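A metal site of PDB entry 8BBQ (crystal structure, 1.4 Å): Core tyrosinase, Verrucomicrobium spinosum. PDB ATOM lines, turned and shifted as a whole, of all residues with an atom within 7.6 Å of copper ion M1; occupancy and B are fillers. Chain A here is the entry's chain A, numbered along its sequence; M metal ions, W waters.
NE2 of His 229 is bound to copper ion M1 (2.0 Å).
Copper ion M1 is bound by a ring nitrogen (NE2) of His 251.
NE2 of His 225 binds copper ion M1 (2.1 Å).
Copper ion M1 is bound by water W1, at 2.2 Å.
Residues that only touch copper ion M1: Phe 247 (3.5 Å) and His 250 (3.9 Å).
Five residues have an atom within 4 Å of copper ion M1: His 225, His 229, Phe 247, His 250 and His 251.
ND1 of His 225 lies within hydrogen-bond range of OD1 of Asn 226 (2.8 Å).
The backbone carbonyl oxygen (O) of His 225 sits at hydrogen-bond distance from a ring nitrogen (NE2) of His 250, 3.3 Å away.
ND1 of His 229 lies within hydrogen-bond range of O of Met 236, at 2.6 Å.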
ATOM      1  N   HIS A  47     -16.275  22.176   2.118  1.00  0.00           N
ATOM      2  CA  HIS A  47     -15.708  22.571   3.439  1.00  0.00           C
ATOM      3  C   HIS A  47     -16.503  23.765   3.993  1.00  0.00           C
ATOM      4  O   HIS A  47     -16.962  23.740   5.146  1.00  0.00           O
ATOM      5  CB  HIS A  47     -14.220  22.850   3.289  1.00  0.00           C
ATOM      6  CG  HIS A  47     -13.528  23.194   4.559  1.00  0.00           C
ATOM      7  ND1 HIS A  47     -13.460  24.465   5.035  1.00  0.00           N
ATOM      8  CD2 HIS A  47     -12.844  22.415   5.444  1.00  0.00           C
ATOM      9  CE1 HIS A  47     -12.756  24.469   6.175  1.00  0.00           C
ATOM     10  NE2 HIS A  47     -12.419  23.236   6.449  1.00  0.00           N
ATOM     11  N   HIS A  53     -16.144  22.680  12.896  1.00  0.00           N
ATOM     12  CA  HIS A  53     -15.007  23.246  13.659  1.00  0.00           C
ATOM     13  C   HIS A  53     -15.444  23.349  15.133  1.00  0.00           C
ATOM     14  O   HIS A  53     -16.621  23.656  15.432  1.00  0.00           O
ATOM     15  CB  HIS A  53     -14.428  24.431  12.836  1.00  0.00           C
ATOM     16  CG  HIS A  53     -14.120  24.025  11.410  1.00  0.00           C
ATOM     17  ND1 HIS A  53     -15.072  24.163  10.394  1.00  0.00           N
ATOM     18  CD2 HIS A  53     -13.047  23.408  10.844  1.00  0.00           C
ATOM     19  CE1 HIS A  53     -14.578  23.651   9.236  1.00  0.00           C
ATOM     20  NE2 HIS A  53     -13.313  23.196   9.488  1.00  0.00           N
ATOM     21  N   PHE A  58     -14.719  16.858  14.298  1.00  0.00           N
ATOM     22  CA  PHE A  58     -13.516  17.440  13.640  1.00  0.00           C
ATOM     23  C   PHE A  58     -12.697  16.386  12.876  1.00  0.00           C
ATOM     24  O   PHE A  58     -12.609  16.421  11.646  1.00  0.00           O
ATOM     25  CB  PHE A  58     -12.684  18.207  14.682  1.00  0.00           C
ATOM     26  CG  PHE A  58     -11.307  18.573  14.201  1.00  0.00           C
ATOM     27  CD1 PHE A  58     -11.156  19.467  13.153  1.00  0.00           C
ATOM     28  CD2 PHE A  58     -10.178  18.053  14.818  1.00  0.00           C
ATOM     29  CE1 PHE A  58      -9.891  19.797  12.698  1.00  0.00           C
ATOM     30  CE2 PHE A  58      -8.903  18.383  14.353  1.00  0.00           C
ATOM     31  CZ  PHE A  58      -8.779  19.250  13.287  1.00  0.00           C
ATOM     32  N   HIS A  62     -13.014  15.329   8.606  1.00  0.00           N
ATOM     33  CA  HIS A  62     -11.808  15.628   7.785  1.00  0.00           C
ATOM     34  C   HIS A  62     -11.251  14.346   7.184  1.00  0.00           C
ATOM     35  O   HIS A  62     -10.686  14.394   6.063  1.00  0.00           O
ATOM     36  CB  HIS A  62     -10.763  16.458   8.565  1.00  0.00           C
ATOM     37  CG  HIS A  62     -11.176  17.913   8.648  1.00  0.00           C
ATOM     38  ND1 HIS A  62     -11.866  18.443   9.718  1.00  0.00           N
ATOM     39  CD2 HIS A  62     -11.061  18.934   7.756  1.00  0.00           C
ATOM     40  CE1 HIS A  62     -12.105  19.739   9.504  1.00  0.00           C
ATOM     41  NE2 HIS A  62     -11.621  20.067   8.296  1.00  0.00           N
ATOM     42  N   HIS A 225      -3.517  22.464  14.610  1.00  0.00           N
ATOM     43  CA  HIS A 225      -4.467  22.609  13.480  1.00  0.00           C
ATOM     44  C   HIS A 225      -4.790  24.088  13.263  1.00  0.00           C
ATOM     45  O   HIS A 225      -4.567  24.572  12.141  1.00  0.00           O
ATOM     46  CB  HIS A 225      -5.729  21.779  13.675  1.00  0.00           C
ATOM     47  CG  HIS A 225      -6.720  22.051  12.590  1.00  0.00           C
ATOM     48  ND1 HIS A 225      -7.803  22.886  12.773  1.00  0.00           N
ATOM     49  CD2 HIS A 225      -6.735  21.640  11.295  1.00  0.00           C
ATOM     50  CE1 HIS A 225      -8.472  22.954  11.638  1.00  0.00           C
ATOM     51  NE2 HIS A 225      -7.818  22.213  10.694  1.00  0.00           N
ATOM     52  N   ASN A 226      -5.371  24.754  14.247  1.00  0.00           N
ATOM     53  CA  ASN A 226      -5.895  26.146  14.109  1.00  0.00           C
ATOM     54  C   ASN A 226      -4.700  27.096  13.877  1.00  0.00           C
ATOM     55  O   ASN A 226      -4.788  27.987  13.030  1.00  0.00           O
ATOM     56  CB  ASN A 226      -6.791  26.536  15.293  1.00  0.00           C
ATOM     57  CG  ASN A 226      -8.148  25.823  15.318  1.00  0.00           C
ATOM     58  OD1 ASN A 226      -8.503  25.099  14.386  1.00  0.00           O
ATOM     59  ND2 ASN A 226      -8.905  26.001  16.411  1.00  0.00           N
ATOM     60  N   HIS A 229      -3.205  26.932  10.319  1.00  0.00           N
ATOM     61  CA  HIS A 229      -4.191  27.585   9.424  1.00  0.00           C
ATOM     62  C   HIS A 229      -3.941  29.104   9.431  1.00  0.00           C
ATOM     63  O   HIS A 229      -3.748  29.735   8.355  1.00  0.00           O
ATOM     64  CB  HIS A 229      -5.625  27.250   9.843  1.00  0.00           C
ATOM     65  CG  HIS A 229      -6.213  26.085   9.112  1.00  0.00           C
ATOM     66  ND1 HIS A 229      -6.718  26.184   7.830  1.00  0.00           N
ATOM     67  CD2 HIS A 229      -6.390  24.793   9.488  1.00  0.00           C
ATOM     68  CE1 HIS A 229      -7.199  24.997   7.467  1.00  0.00           C
ATOM     69  NE2 HIS A 229      -6.977  24.138   8.426  1.00  0.00           N
ATOM     70  N   MET A 236      -6.113  29.951   3.851  1.00  0.00           N
ATOM     71  CA  MET A 236      -5.989  28.958   4.931  1.00  0.00           C
ATOM     72  C   MET A 236      -6.560  29.520   6.242  1.00  0.00           C
ATOM     73  O   MET A 236      -6.768  28.722   7.131  1.00  0.00           O
ATOM     74  CB  MET A 236      -4.541  28.467   5.100  1.00  0.00           C
ATOM     75  CG  MET A 236      -4.171  27.465   4.034  1.00  0.00           C
ATOM     76  SD  MET A 236      -5.003  25.849   4.287  1.00  0.00           S
ATOM     77  CE  MET A 236      -4.091  25.175   5.655  1.00  0.00           C
ATOM     78  N   ASP A 238      -9.512  30.849   6.738  1.00  0.00           N
ATOM     79  CA  ASP A 238     -10.998  30.857   6.774  1.00  0.00           C
ATOM     80  C   ASP A 238     -11.568  29.678   5.990  1.00  0.00           C
ATOM     81  O   ASP A 238     -10.789  28.764   5.595  1.00  0.00           O
ATOM     82  CB  ASP A 238     -11.510  32.240   6.346  1.00  0.00           C
ATOM     83  CG  ASP A 238     -12.729  32.692   7.147  1.00  0.00           C
ATOM     84  OD1 ASP A 238     -13.653  31.876   7.333  1.00  0.00           O
ATOM     85  OD2 ASP A 238     -12.725  33.872   7.578  1.00  0.00           O
ATOM     86  N   SER A 241     -10.440  27.528   2.940  1.00  0.00           N
ATOM     87  CA  SER A 241      -9.061  26.993   3.120  1.00  0.00           C
ATOM     88  C   SER A 241      -8.680  25.907   2.102  1.00  0.00           C
ATOM     89  O   SER A 241      -7.530  25.928   1.678  1.00  0.00           O
ATOM     90  CB  SER A 241      -8.817  26.539   4.528  1.00  0.00           C
ATOM     91  OG  SER A 241      -9.852  25.700   5.033  1.00  0.00           O
ATOM     92  N   PRO A 242      -9.557  24.948   1.665  1.00  0.00           N
ATOM     93  CA  PRO A 242      -9.144  23.951   0.678  1.00  0.00           C
ATOM     94  C   PRO A 242      -8.834  24.506  -0.717  1.00  0.00           C
ATOM     95  O   PRO A 242      -8.361  23.763  -1.555  1.00  0.00           O
ATOM     96  CB  PRO A 242     -10.288  22.940   0.601  1.00  0.00           C
ATOM     97  CG  PRO A 242     -11.070  23.189   1.914  1.00  0.00           C
ATOM     98  CD  PRO A 242     -10.919  24.684   2.170  1.00  0.00           C
ATOM     99  N   PHE A 247      -3.704  22.635   2.108  1.00  0.00           N
ATOM    100  CA  PHE A 247      -4.794  22.185   3.008  1.00  0.00           C
ATOM    101  C   PHE A 247      -4.756  20.659   3.126  1.00  0.00           C
ATOM    102  O   PHE A 247      -4.812  20.146   4.241  1.00  0.00           O
ATOM    103  CB  PHE A 247      -6.163  22.630   2.498  1.00  0.00           C
ATOM    104  CG  PHE A 247      -7.304  22.112   3.335  1.00  0.00           C
ATOM    105  CD1 PHE A 247      -7.871  20.878   3.099  1.00  0.00           C
ATOM    106  CD2 PHE A 247      -7.800  22.878   4.366  1.00  0.00           C
ATOM    107  CE1 PHE A 247      -8.946  20.437   3.859  1.00  0.00           C
ATOM    108  CE2 PHE A 247      -8.861  22.440   5.130  1.00  0.00           C
ATOM    109  CZ  PHE A 247      -9.453  21.231   4.856  1.00  0.00           C
ATOM    110  N   HIS A 250      -1.706  19.369   5.072  1.00  0.00           N
ATOM    111  CA  HIS A 250      -2.009  19.701   6.484  1.00  0.00           C
ATOM    112  C   HIS A 250      -2.934  18.629   7.044  1.00  0.00           C
ATOM    113  O   HIS A 250      -2.624  18.050   8.111  1.00  0.00           O
ATOM    114  CB  HIS A 250      -2.604  21.123   6.570  1.00  0.00           C
ATOM    115  CG  HIS A 250      -2.981  21.578   7.939  1.00  0.00           C
ATOM    116  ND1 HIS A 250      -2.123  21.480   8.989  1.00  0.00           N
ATOM    117  CD2 HIS A 250      -4.086  22.209   8.398  1.00  0.00           C
ATOM    118  CE1 HIS A 250      -2.692  22.005  10.063  1.00  0.00           C
ATOM    119  NE2 HIS A 250      -3.895  22.467   9.743  1.00  0.00           N
ATOM    120  N   HIS A 251      -4.017  18.307   6.329  1.00  0.00           N
ATOM    121  CA  HIS A 251      -5.034  17.351   6.858  1.00  0.00           C
ATOM    122  C   HIS A 251      -4.566  15.908   6.760  1.00  0.00           C
ATOM    123  O   HIS A 251      -4.993  15.078   7.600  1.00  0.00           O
ATOM    124  CB  HIS A 251      -6.412  17.601   6.241  1.00  0.00           C
ATOM    125  CG  HIS A 251      -7.104  18.621   7.060  1.00  0.00           C
ATOM    126  ND1 HIS A 251      -7.715  18.330   8.286  1.00  0.00           N
ATOM    127  CD2 HIS A 251      -7.113  19.962   6.950  1.00  0.00           C
ATOM    128  CE1 HIS A 251      -8.109  19.464   8.850  1.00  0.00           C
ATOM    129  NE2 HIS A 251      -7.807  20.448   8.015  1.00  0.00           N
ATOM    130  N   ILE A 254      -2.810  15.775  10.068  1.00  0.00           N
ATOM    131  CA  ILE A 254      -3.810  15.678  11.168  1.00  0.00           C
ATOM    132  C   ILE A 254      -4.346  14.243  11.233  1.00  0.00           C
ATOM    133  O   ILE A 254      -4.427  13.667  12.294  1.00  0.00           O
ATOM    134  CB  ILE A 254      -4.925  16.701  10.986  1.00  0.00           C
ATOM    135  CG1 ILE A 254      -4.416  18.158  11.130  1.00  0.00           C
ATOM    136  CG2 ILE A 254      -6.127  16.398  11.874  1.00  0.00           C
ATOM    137  CD1 ILE A 254      -4.005  18.535  12.511  1.00  0.00           C
HETATM  138 CU    CU M   1      -7.975  22.401   8.566  1.00  0.00          CU
HETATM  139 CU    CU M   2     -11.907  22.215   8.231  1.00  0.00          CU
HETATM  140  O   HOH W   1     -10.095  23.132   8.536  1.00  0.00           O
